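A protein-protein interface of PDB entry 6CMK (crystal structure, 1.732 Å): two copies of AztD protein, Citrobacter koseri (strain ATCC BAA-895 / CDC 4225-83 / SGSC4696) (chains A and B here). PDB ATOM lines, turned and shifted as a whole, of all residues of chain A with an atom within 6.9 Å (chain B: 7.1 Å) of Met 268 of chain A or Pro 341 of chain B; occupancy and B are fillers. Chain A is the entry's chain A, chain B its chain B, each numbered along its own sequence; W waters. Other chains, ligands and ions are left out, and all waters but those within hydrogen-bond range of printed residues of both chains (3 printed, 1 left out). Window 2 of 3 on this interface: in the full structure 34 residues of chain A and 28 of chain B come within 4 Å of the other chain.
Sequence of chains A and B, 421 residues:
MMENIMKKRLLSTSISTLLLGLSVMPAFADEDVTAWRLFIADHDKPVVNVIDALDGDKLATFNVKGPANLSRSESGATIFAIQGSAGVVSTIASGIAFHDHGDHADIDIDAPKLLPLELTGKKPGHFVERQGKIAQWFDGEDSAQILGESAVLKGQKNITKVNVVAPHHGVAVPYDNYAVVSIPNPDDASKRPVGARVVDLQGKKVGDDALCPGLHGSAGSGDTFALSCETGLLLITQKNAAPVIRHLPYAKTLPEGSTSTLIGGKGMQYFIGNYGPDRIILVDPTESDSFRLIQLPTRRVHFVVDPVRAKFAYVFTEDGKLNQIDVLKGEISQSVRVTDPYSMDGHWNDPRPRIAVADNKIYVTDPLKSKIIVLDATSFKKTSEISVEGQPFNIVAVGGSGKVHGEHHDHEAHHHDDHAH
The backbone NH (N) of Asp 319 of chain B sits close to the backbone carbonyl oxygen (O) of Gly 267 of chain A, 3.3 Å away. The backbone carbonyl oxygen of Lys 266 of chain A lies close to the side-chain carboxylate of Glu 318 of chain B (3.3 Å). O of Gly 267 of chain A sits close to O of Glu 318 of chain B, 3.3 Å away.
The side-chain carboxylate (OD2) of Asp 319 of chain B lies within hydrogen-bond range of the side-chain hydroxyl (OG1) of Thr 298 of chain B, 2.9 Å away. OG of Ser 343 of chain B sits at hydrogen-bond distance from NH2 of Arg 299 of chain B (3.4 Å). The side-chain hydroxyl (OG1) of Thr 317 of chain B is in hydrogen-bond range of the side-chain carboxylate (OD1) of Asp 319 of chain B (2.6 Å). O of Glu 318 of chain B is in hydrogen-bond range of N of Tyr 342 of chain B, at 2.8 Å. The side-chain hydroxyl (OG) of Ser 221 of chain A is in hydrogen-bond range of the backbone carbonyl oxygen (O) of Met 268 of chain A (3.4 Å). O of Ser 221 of chain A sits at hydrogen-bond distance from NE2 of Gln 269 of chain A (3.0 Å).
Among the printed residues, pairs that only touch across the chains: Val 308 of chain A with Ser 343 of chain B (3.5 Å), Gln 269 of chain A with Thr 298 of chain B (3.6 Å), Met 268 of chain A with Pro 341 of chain B (3.8 Å), Ala 310 of chain A with Pro 341 of chain B (3.8 Å) and Lys 266 of chain A with Arg 299 of chain B (3.8 Å).
Of the printed residues of chain B, Lys 266 of chain A touches Arg 299 (3.8 Å) and Glu 318 (3.3 Å). Of chain B, only Glu 318 and Asp 319 come within 4 Å of Gly 267 of chain A. Of the printed residues of chain B, Met 268 of chain A touches Pro 341. Arg 309 of chain A touches none of the printed residues of chain B. Of the printed residues of chain A, Arg 299 of chain B touches Lys 266 (3.8 Å). Printed residues of chain A within 4 Å of Pro 341 of chain B: Met 268 and Ala 310. The nearest residue of chain A that does not touch Pro 341 of chain B is Gly 267 of chain A (4.1 Å). The nearest printed residue of chain B that does not touch Val 308 of chain A is Tyr 342 of chain B (5.8 Å).
Hydrophobic or aromatic side chains of chain A that line the printed part of chain B: Met 268 and Ala 310. Among the printed residues, 8 pairs touch across the chains.
No position is printed for both chains. Of the 8 pairs that touch across the chains among the printed residues, none has its exchanged pair printed and touching as well.
Water W1 lies within hydrogen-bond range of the side-chain carboxylate of Glu 318 of chain B (2.6 Å) and the backbone carbonyl oxygen of Lys 266 of chain A (2.7 Å). Water W2 lies within hydrogen-bond range of OE1 of Gln 269 of chain A, OD2 of Asp 319 of chain B and NZ of Lys 321 of chain B. Water W3 lies within hydrogen-bond range of O of Val 308 of chain A (2.8 Å), N of Ser 343 of chain B (3.1 Å) and N of Ala 310 of chain A (3.1 Å).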
ATOM      1  N   SER A 221     -21.531  -4.883 -37.414  1.00  0.00           N
ATOM      2  CA  SER A 221     -20.659  -4.556 -36.289  1.00  0.00           C
ATOM      3  C   SER A 221     -20.251  -3.098 -36.454  1.00  0.00           C
ATOM      4  O   SER A 221     -19.464  -2.766 -37.345  1.00  0.00           O
ATOM      5  CB  SER A 221     -19.445  -5.473 -36.248  1.00  0.00           C
ATOM      6  OG  SER A 221     -18.651  -5.211 -35.088  1.00  0.00           O
ATOM      7  N   GLY A 222     -20.775  -2.240 -35.590  1.00  0.00           N
ATOM      8  CA  GLY A 222     -20.520  -0.817 -35.765  1.00  0.00           C
ATOM      9  C   GLY A 222     -20.989  -0.368 -37.129  1.00  0.00           C
ATOM     10  O   GLY A 222     -22.072  -0.741 -37.589  1.00  0.00           O
ATOM     11  N   GLY A 264     -21.815 -10.198 -35.102  1.00  0.00           N
ATOM     12  CA  GLY A 264     -20.979  -9.000 -35.087  1.00  0.00           C
ATOM     13  C   GLY A 264     -20.790  -8.431 -33.695  1.00  0.00           C
ATOM     14  O   GLY A 264     -21.739  -8.354 -32.910  1.00  0.00           O
ATOM     15  N   GLY A 265     -19.561  -8.012 -33.408  1.00  0.00           N
ATOM     16  CA  GLY A 265     -19.271  -7.394 -32.125  1.00  0.00           C
ATOM     17  C   GLY A 265     -20.045  -6.105 -31.924  1.00  0.00           C
ATOM     18  O   GLY A 265     -20.361  -5.385 -32.871  1.00  0.00           O
ATOM     19  N   LYS A 266     -20.349  -5.802 -30.665  1.00  0.00           N
ATOM     20  CA  LYS A 266     -21.105  -4.586 -30.370  1.00  0.00           C
ATOM     21  C   LYS A 266     -20.227  -3.427 -29.922  1.00  0.00           C
ATOM     22  O   LYS A 266     -20.318  -2.331 -30.488  1.00  0.00           O
ATOM     23  CB  LYS A 266     -22.177  -4.867 -29.313  1.00  0.00           C
ATOM     24  CG  LYS A 266     -23.513  -5.270 -29.914  1.00  0.00           C
ATOM     25  CD  LYS A 266     -24.601  -4.232 -29.658  1.00  0.00           C
ATOM     26  CE  LYS A 266     -24.292  -2.879 -30.293  1.00  0.00           C
ATOM     27  NZ  LYS A 266     -25.532  -2.192 -30.767  1.00  0.00           N
ATOM     28  N   GLY A 267     -19.377  -3.637 -28.922  1.00  0.00           N
ATOM     29  CA  GLY A 267     -18.534  -2.566 -28.425  1.00  0.00           C
ATOM     30  C   GLY A 267     -17.204  -2.451 -29.123  1.00  0.00           C
ATOM     31  O   GLY A 267     -16.498  -1.452 -28.984  1.00  0.00           O
ATOM     32  N   MET A 268     -16.867  -3.470 -29.895  1.00  0.00           N
ATOM     33  CA  MET A 268     -15.638  -3.568 -30.654  1.00  0.00           C
ATOM     34  C   MET A 268     -16.047  -4.094 -32.022  1.00  0.00           C
ATOM     35  O   MET A 268     -17.002  -4.865 -32.119  1.00  0.00           O
ATOM     36  CB  MET A 268     -14.679  -4.514 -29.909  1.00  0.00           C
ATOM     37  CG  MET A 268     -13.341  -4.824 -30.524  1.00  0.00           C
ATOM     38  SD  MET A 268     -12.389  -5.727 -29.266  1.00  0.00           S
ATOM     39  CE  MET A 268     -12.921  -7.414 -29.520  1.00  0.00           C
ATOM     40  N   GLN A 269     -15.364  -3.655 -33.085  1.00  0.00           N
ATOM     41  CA  GLN A 269     -15.733  -4.075 -34.439  1.00  0.00           C
ATOM     42  C   GLN A 269     -15.031  -5.374 -34.809  1.00  0.00           C
ATOM     43  O   GLN A 269     -13.804  -5.404 -34.968  1.00  0.00           O
ATOM     44  CB  GLN A 269     -15.417  -2.992 -35.464  1.00  0.00           C
ATOM     45  CG  GLN A 269     -16.367  -1.828 -35.372  1.00  0.00           C
ATOM     46  CD  GLN A 269     -16.212  -0.868 -36.530  1.00  0.00           C
ATOM     47  OE1 GLN A 269     -15.293  -0.054 -36.557  1.00  0.00           O
ATOM     48  NE2 GLN A 269     -17.095  -0.988 -37.515  1.00  0.00           N
ATOM     49  N   TYR A 270     -15.819  -6.440 -34.973  1.00  0.00           N
ATOM     50  CA  TYR A 270     -15.326  -7.716 -35.470  1.00  0.00           C
ATOM     51  C   TYR A 270     -16.524  -8.549 -35.891  1.00  0.00           C
ATOM     52  O   TYR A 270     -17.663  -8.262 -35.522  1.00  0.00           O
ATOM     53  CB  TYR A 270     -14.502  -8.475 -34.413  1.00  0.00           C
ATOM     54  CG  TYR A 270     -15.303  -8.957 -33.222  1.00  0.00           C
ATOM     55  CD1 TYR A 270     -15.462  -8.164 -32.087  1.00  0.00           C
ATOM     56  CD2 TYR A 270     -15.903 -10.208 -33.227  1.00  0.00           C
ATOM     57  CE1 TYR A 270     -16.190  -8.613 -30.992  1.00  0.00           C
ATOM     58  CE2 TYR A 270     -16.633 -10.654 -32.149  1.00  0.00           C
ATOM     59  CZ  TYR A 270     -16.768  -9.866 -31.033  1.00  0.00           C
ATOM     60  OH  TYR A 270     -17.500 -10.320 -29.973  1.00  0.00           O
ATOM     61  N   PHE A 271     -16.242  -9.620 -36.636  1.00  0.00           N
ATOM     62  CA  PHE A 271     -17.241 -10.619 -36.953  1.00  0.00           C
ATOM     63  C   PHE A 271     -16.731 -11.983 -36.528  1.00  0.00           C
ATOM     64  O   PHE A 271     -15.526 -12.239 -36.524  1.00  0.00           O
ATOM     65  CB  PHE A 271     -17.580 -10.608 -38.446  1.00  0.00           C
ATOM     66  CG  PHE A 271     -18.126  -9.304 -38.906  1.00  0.00           C
ATOM     67  CD1 PHE A 271     -19.442  -8.982 -38.660  1.00  0.00           C
ATOM     68  CD2 PHE A 271     -17.313  -8.381 -39.544  1.00  0.00           C
ATOM     69  CE1 PHE A 271     -19.951  -7.760 -39.047  1.00  0.00           C
ATOM     70  CE2 PHE A 271     -17.816  -7.160 -39.942  1.00  0.00           C
ATOM     71  CZ  PHE A 271     -19.135  -6.846 -39.694  1.00  0.00           C
ATOM     72  N   VAL A 308     -21.830  -6.221 -23.442  1.00  0.00           N
ATOM     73  CA  VAL A 308     -21.349  -5.440 -22.308  1.00  0.00           C
ATOM     74  C   VAL A 308     -19.838  -5.563 -22.151  1.00  0.00           C
ATOM     75  O   VAL A 308     -19.140  -4.564 -21.949  1.00  0.00           O
ATOM     76  CB  VAL A 308     -22.096  -5.887 -21.030  1.00  0.00           C
ATOM     77  CG1 VAL A 308     -21.562  -5.150 -19.804  1.00  0.00           C
ATOM     78  CG2 VAL A 308     -23.587  -5.658 -21.165  1.00  0.00           C
ATOM     79  N   ARG A 309     -19.309  -6.789 -22.209  1.00  0.00           N
ATOM     80  CA  ARG A 309     -17.871  -7.042 -22.142  1.00  0.00           C
ATOM     81  C   ARG A 309     -17.393  -7.303 -23.568  1.00  0.00           C
ATOM     82  O   ARG A 309     -17.396  -8.431 -24.059  1.00  0.00           O
ATOM     83  CB  ARG A 309     -17.563  -8.198 -21.198  1.00  0.00           C
ATOM     84  CG  ARG A 309     -17.951  -7.919 -19.750  1.00  0.00           C
ATOM     85  CD  ARG A 309     -18.433  -9.178 -19.039  1.00  0.00           C
ATOM     86  NE  ARG A 309     -19.775  -9.507 -19.517  1.00  0.00           N
ATOM     87  CZ  ARG A 309     -20.899  -9.013 -19.002  1.00  0.00           C
ATOM     88  NH1 ARG A 309     -20.864  -8.197 -17.941  1.00  0.00           N
ATOM     89  NH2 ARG A 309     -22.061  -9.353 -19.533  1.00  0.00           N
ATOM     90  N   ALA A 310     -16.951  -6.239 -24.232  1.00  0.00           N
ATOM     91  CA  ALA A 310     -16.669  -6.298 -25.660  1.00  0.00           C
ATOM     92  C   ALA A 310     -15.559  -7.271 -26.034  1.00  0.00           C
ATOM     93  O   ALA A 310     -15.477  -7.662 -27.199  1.00  0.00           O
ATOM     94  CB  ALA A 310     -16.288  -4.909 -26.178  1.00  0.00           C
ATOM     95  N   LYS A 311     -14.680  -7.642 -25.107  1.00  0.00           N
ATOM     96  CA  LYS A 311     -13.605  -8.547 -25.481  1.00  0.00           C
ATOM     97  C   LYS A 311     -14.058 -10.000 -25.607  1.00  0.00           C
ATOM     98  O   LYS A 311     -13.243 -10.840 -25.992  1.00  0.00           O
ATOM     99  CB  LYS A 311     -12.463  -8.460 -24.469  1.00  0.00           C
ATOM    100  CG  LYS A 311     -12.813  -8.909 -23.067  1.00  0.00           C
ATOM    101  CD  LYS A 311     -11.573  -9.187 -22.231  1.00  0.00           C
ATOM    102  CE  LYS A 311     -10.631  -7.997 -22.156  1.00  0.00           C
ATOM    103  NZ  LYS A 311      -9.217  -8.421 -22.322  1.00  0.00           N
ATOM    104  N   PHE A 312     -15.316 -10.316 -25.306  1.00  0.00           N
ATOM    105  CA  PHE A 312     -15.757 -11.701 -25.212  1.00  0.00           C
ATOM    106  C   PHE A 312     -16.926 -11.991 -26.145  1.00  0.00           C
ATOM    107  O   PHE A 312     -17.753 -11.119 -26.435  1.00  0.00           O
ATOM    108  CB  PHE A 312     -16.157 -12.049 -23.778  1.00  0.00           C
ATOM    109  CG  PHE A 312     -14.991 -12.111 -22.833  1.00  0.00           C
ATOM    110  CD1 PHE A 312     -13.989 -13.041 -23.025  1.00  0.00           C
ATOM    111  CD2 PHE A 312     -14.891 -11.236 -21.766  1.00  0.00           C
ATOM    112  CE1 PHE A 312     -12.907 -13.105 -22.174  1.00  0.00           C
ATOM    113  CE2 PHE A 312     -13.809 -11.293 -20.907  1.00  0.00           C
ATOM    114  CZ  PHE A 312     -12.816 -12.230 -21.112  1.00  0.00           C
ATOM    115  N   VAL A 327     -11.762 -12.733 -27.752  1.00  0.00           N
ATOM    116  CA  VAL A 327     -11.674 -12.330 -29.151  1.00  0.00           C
ATOM    117  C   VAL A 327     -10.301 -11.751 -29.470  1.00  0.00           C
ATOM    118  O   VAL A 327      -9.750 -11.984 -30.552  1.00  0.00           O
ATOM    119  CB  VAL A 327     -12.809 -11.340 -29.477  1.00  0.00           C
ATOM    120  CG1 VAL A 327     -12.715 -10.850 -30.901  1.00  0.00           C
ATOM    121  CG2 VAL A 327     -14.157 -12.014 -29.251  1.00  0.00           C
ATOM    122  N   LEU A 328      -9.722 -10.992 -28.543  1.00  0.00           N
ATOM    123  CA  LEU A 328      -8.412 -10.400 -28.804  1.00  0.00           C
ATOM    124  C   LEU A 328      -7.295 -11.436 -28.766  1.00  0.00           C
ATOM    125  O   LEU A 328      -6.333 -11.329 -29.534  1.00  0.00           O
ATOM    126  CB  LEU A 328      -8.158  -9.267 -27.809  1.00  0.00           C
ATOM    127  CG  LEU A 328      -9.173  -8.138 -28.054  1.00  0.00           C
ATOM    128  CD1 LEU A 328      -9.180  -7.100 -26.945  1.00  0.00           C
ATOM    129  CD2 LEU A 328      -8.913  -7.463 -29.399  1.00  0.00           C
ATOM    130  N   THR B 298     -18.167   3.210 -34.117  1.00  0.00           N
ATOM    131  CA  THR B 298     -18.965   2.582 -33.076  1.00  0.00           C
ATOM    132  C   THR B 298     -19.629   3.715 -32.295  1.00  0.00           C
ATOM    133  O   THR B 298     -19.542   4.889 -32.677  1.00  0.00           O
ATOM    134  CB  THR B 298     -18.118   1.660 -32.174  1.00  0.00           C
ATOM    135  OG1 THR B 298     -16.985   2.366 -31.675  1.00  0.00           O
ATOM    136  CG2 THR B 298     -17.620   0.443 -32.940  1.00  0.00           C
ATOM    137  N   ARG B 299     -20.332   3.364 -31.220  1.00  0.00           N
ATOM    138  CA  ARG B 299     -21.119   4.364 -30.509  1.00  0.00           C
ATOM    139  C   ARG B 299     -20.229   5.374 -29.789  1.00  0.00           C
ATOM    140  O   ARG B 299     -19.143   5.061 -29.299  1.00  0.00           O
ATOM    141  CB  ARG B 299     -22.068   3.715 -29.504  1.00  0.00           C
ATOM    142  CG  ARG B 299     -23.202   2.930 -30.179  1.00  0.00           C
ATOM    143  CD  ARG B 299     -24.031   2.142 -29.175  1.00  0.00           C
ATOM    144  NE  ARG B 299     -23.241   1.057 -28.619  1.00  0.00           N
ATOM    145  CZ  ARG B 299     -23.715   0.090 -27.841  1.00  0.00           C
ATOM    146  NH1 ARG B 299     -25.003   0.053 -27.515  1.00  0.00           N
ATOM    147  NH2 ARG B 299     -22.887  -0.846 -27.388  1.00  0.00           N
ATOM    148  N   PHE B 316     -14.673  10.365 -28.906  1.00  0.00           N
ATOM    149  CA  PHE B 316     -14.175   9.099 -28.395  1.00  0.00           C
ATOM    150  C   PHE B 316     -15.287   8.077 -28.528  1.00  0.00           C
ATOM    151  O   PHE B 316     -16.427   8.347 -28.139  1.00  0.00           O
ATOM    152  CB  PHE B 316     -13.738   9.213 -26.938  1.00  0.00           C
ATOM    153  CG  PHE B 316     -12.892   8.059 -26.498  1.00  0.00           C
ATOM    154  CD1 PHE B 316     -13.463   6.933 -25.956  1.00  0.00           C
ATOM    155  CD2 PHE B 316     -11.523   8.087 -26.705  1.00  0.00           C
ATOM    156  CE1 PHE B 316     -12.679   5.862 -25.602  1.00  0.00           C
ATOM    157  CE2 PHE B 316     -10.731   7.022 -26.339  1.00  0.00           C
ATOM    158  CZ  PHE B 316     -11.321   5.909 -25.789  1.00  0.00           C
ATOM    159  N   THR B 317     -14.966   6.924 -29.110  1.00  0.00           N
ATOM    160  CA  THR B 317     -15.954   5.889 -29.367  1.00  0.00           C
ATOM    161  C   THR B 317     -15.687   4.645 -28.515  1.00  0.00           C
ATOM    162  O   THR B 317     -14.601   4.458 -27.942  1.00  0.00           O
ATOM    163  CB  THR B 317     -16.014   5.565 -30.872  1.00  0.00           C
ATOM    164  OG1 THR B 317     -14.715   5.463 -31.452  1.00  0.00           O
ATOM    165  CG2 THR B 317     -16.751   6.699 -31.599  1.00  0.00           C
ATOM    166  N   GLU B 318     -16.733   3.829 -28.383  1.00  0.00           N
ATOM    167  CA  GLU B 318     -16.714   2.699 -27.455  1.00  0.00           C
ATOM    168  C   GLU B 318     -15.675   1.651 -27.819  1.00  0.00           C
ATOM    169  O   GLU B 318     -15.274   0.867 -26.941  1.00  0.00           O
ATOM    170  CB  GLU B 318     -18.102   2.073 -27.388  1.00  0.00           C
ATOM    171  CG  GLU B 318     -18.567   1.513 -28.702  1.00  0.00           C
ATOM    172  CD  GLU B 318     -19.931   0.873 -28.625  1.00  0.00           C
ATOM    173  OE1 GLU B 318     -20.621   0.827 -29.679  1.00  0.00           O
ATOM    174  OE2 GLU B 318     -20.303   0.391 -27.526  1.00  0.00           O
ATOM    175  N   ASP B 319     -15.212   1.639 -29.067  1.00  0.00           N
ATOM    176  CA  ASP B 319     -14.140   0.758 -29.504  1.00  0.00           C
ATOM    177  C   ASP B 319     -12.795   1.131 -28.908  1.00  0.00           C
ATOM    178  O   ASP B 319     -11.820   0.404 -29.133  1.00  0.00           O
ATOM    179  CB  ASP B 319     -14.043   0.732 -31.039  1.00  0.00           C
ATOM    180  CG  ASP B 319     -14.022   2.125 -31.672  1.00  0.00           C
ATOM    181  OD1 ASP B 319     -13.645   3.095 -30.986  1.00  0.00           O
ATOM    182  OD2 ASP B 319     -14.376   2.251 -32.871  1.00  0.00           O
ATOM    183  N   GLY B 320     -12.724   2.212 -28.132  1.00  0.00           N
ATOM    184  CA  GLY B 320     -11.479   2.672 -27.563  1.00  0.00           C
ATOM    185  C   GLY B 320     -10.705   3.646 -28.417  1.00  0.00           C
ATOM    186  O   GLY B 320      -9.552   3.934 -28.096  1.00  0.00           O
ATOM    187  N   LYS B 321     -11.292   4.159 -29.492  1.00  0.00           N
ATOM    188  CA  LYS B 321     -10.577   5.038 -30.405  1.00  0.00           C
ATOM    189  C   LYS B 321     -10.951   6.497 -30.195  1.00  0.00           C
ATOM    190  O   LYS B 321     -12.094   6.837 -29.880  1.00  0.00           O
ATOM    191  CB  LYS B 321     -10.860   4.666 -31.860  1.00  0.00           C
ATOM    192  CG  LYS B 321     -10.387   3.272 -32.231  1.00  0.00           C
ATOM    193  CD  LYS B 321     -10.770   2.938 -33.664  1.00  0.00           C
ATOM    194  CE  LYS B 321     -10.451   1.496 -33.998  1.00  0.00           C
ATOM    195  NZ  LYS B 321     -10.952   1.146 -35.355  1.00  0.00           N
ATOM    196  N   ARG B 337      -6.396   4.106 -31.787  1.00  0.00           N
ATOM    197  CA  ARG B 337      -6.786   3.371 -30.595  1.00  0.00           C
ATOM    198  C   ARG B 337      -6.042   3.921 -29.385  1.00  0.00           C
ATOM    199  O   ARG B 337      -4.816   4.080 -29.411  1.00  0.00           O
ATOM    200  CB  ARG B 337      -6.501   1.874 -30.770  1.00  0.00           C
ATOM    201  CG  ARG B 337      -6.718   1.061 -29.497  1.00  0.00           C
ATOM    202  CD  ARG B 337      -6.741  -0.443 -29.752  1.00  0.00           C
ATOM    203  NE  ARG B 337      -7.855  -0.848 -30.608  1.00  0.00           N
ATOM    204  CZ  ARG B 337      -7.767  -1.080 -31.914  1.00  0.00           C
ATOM    205  NH1 ARG B 337      -6.609  -0.957 -32.551  1.00  0.00           N
ATOM    206  NH2 ARG B 337      -8.847  -1.444 -32.591  1.00  0.00           N
ATOM    207  N   THR B 339      -7.624   3.360 -25.741  1.00  0.00           N
ATOM    208  CA  THR B 339      -7.925   2.489 -24.611  1.00  0.00           C
ATOM    209  C   THR B 339      -8.432   1.140 -25.108  1.00  0.00           C
ATOM    210  O   THR B 339      -8.678   0.926 -26.300  1.00  0.00           O
ATOM    211  CB  THR B 339      -8.973   3.107 -23.660  1.00  0.00           C
ATOM    212  OG1 THR B 339     -10.247   3.180 -24.314  1.00  0.00           O
ATOM    213  CG2 THR B 339      -8.578   4.505 -23.210  1.00  0.00           C
ATOM    214  N   ASP B 340      -8.565   0.205 -24.160  1.00  0.00           N
ATOM    215  CA  ASP B 340      -9.413  -0.948 -24.378  1.00  0.00           C
ATOM    216  C   ASP B 340     -10.845  -0.493 -24.665  1.00  0.00           C
ATOM    217  O   ASP B 340     -11.237   0.638 -24.347  1.00  0.00           O
ATOM    218  CB  ASP B 340      -9.402  -1.870 -23.157  1.00  0.00           C
ATOM    219  CG  ASP B 340      -8.089  -2.614 -22.992  1.00  0.00           C
ATOM    220  OD1 ASP B 340      -7.294  -2.663 -23.952  1.00  0.00           O
ATOM    221  OD2 ASP B 340      -7.864  -3.161 -21.896  1.00  0.00           O
ATOM    222  N   PRO B 341     -11.657  -1.367 -25.241  1.00  0.00           N
ATOM    223  CA  PRO B 341     -13.058  -1.018 -25.476  1.00  0.00           C
ATOM    224  C   PRO B 341     -13.805  -0.739 -24.180  1.00  0.00           C
ATOM    225  O   PRO B 341     -13.574  -1.367 -23.143  1.00  0.00           O
ATOM    226  CB  PRO B 341     -13.621  -2.258 -26.187  1.00  0.00           C
ATOM    227  CG  PRO B 341     -12.417  -2.972 -26.716  1.00  0.00           C
ATOM    228  CD  PRO B 341     -11.343  -2.724 -25.712  1.00  0.00           C
ATOM    229  N   TYR B 342     -14.748   0.198 -24.275  1.00  0.00           N
ATOM    230  CA  TYR B 342     -15.671   0.563 -23.203  1.00  0.00           C
ATOM    231  C   TYR B 342     -17.062   0.569 -23.822  1.00  0.00           C
ATOM    232  O   TYR B 342     -17.543   1.622 -24.240  1.00  0.00           O
ATOM    233  CB  TYR B 342     -15.334   1.929 -22.630  1.00  0.00           C
ATOM    234  CG  TYR B 342     -14.245   2.047 -21.573  1.00  0.00           C
ATOM    235  CD1 TYR B 342     -12.932   2.282 -21.928  1.00  0.00           C
ATOM    236  CD2 TYR B 342     -14.556   2.005 -20.223  1.00  0.00           C
ATOM    237  CE1 TYR B 342     -11.953   2.452 -20.964  1.00  0.00           C
ATOM    238  CE2 TYR B 342     -13.580   2.174 -19.252  1.00  0.00           C
ATOM    239  CZ  TYR B 342     -12.291   2.395 -19.631  1.00  0.00           C
ATOM    240  OH  TYR B 342     -11.325   2.580 -18.670  1.00  0.00           O
ATOM    241  N   SER B 343     -17.697  -0.598 -23.913  1.00  0.00           N
ATOM    242  CA  SER B 343     -19.019  -0.664 -24.517  1.00  0.00           C
ATOM    243  C   SER B 343     -19.979   0.318 -23.859  1.00  0.00           C
ATOM    244  O   SER B 343     -19.965   0.518 -22.643  1.00  0.00           O
ATOM    245  CB  SER B 343     -19.599  -2.072 -24.386  1.00  0.00           C
ATOM    246  OG  SER B 343     -20.896  -2.095 -24.933  1.00  0.00           O
ATOM    247  N   PRO B 353     -14.197   6.610 -20.592  1.00  0.00           N
ATOM    248  CA  PRO B 353     -13.305   7.745 -20.862  1.00  0.00           C
ATOM    249  C   PRO B 353     -14.023   9.057 -21.138  1.00  0.00           C
ATOM    250  O   PRO B 353     -15.153   9.090 -21.633  1.00  0.00           O
ATOM    251  CB  PRO B 353     -12.528   7.291 -22.098  1.00  0.00           C
ATOM    252  CG  PRO B 353     -12.481   5.829 -21.963  1.00  0.00           C
ATOM    253  CD  PRO B 353     -13.827   5.447 -21.416  1.00  0.00           C
ATOM    254  N   LEU B 368     -10.718   2.698 -15.658  1.00  0.00           N
ATOM    255  CA  LEU B 368     -10.477   1.346 -15.170  1.00  0.00           C
ATOM    256  C   LEU B 368      -9.002   0.999 -15.083  1.00  0.00           C
ATOM    257  O   LEU B 368      -8.664  -0.007 -14.448  1.00  0.00           O
ATOM    258  CB  LEU B 368     -11.197   0.345 -16.060  1.00  0.00           C
ATOM    259  CG  LEU B 368     -12.725   0.381 -15.981  1.00  0.00           C
ATOM    260  CD1 LEU B 368     -13.296  -0.626 -16.955  1.00  0.00           C
ATOM    261  CD2 LEU B 368     -13.221   0.103 -14.559  1.00  0.00           C
HETATM  262  O   HOH W   1     -21.220  -0.276 -31.939  1.00  0.00           O
HETATM  263  O   HOH W   2     -13.614   0.375 -34.630  1.00  0.00           O
HETATM  264  O   HOH W   3     -16.757  -3.399 -22.956  1.00  0.00           O
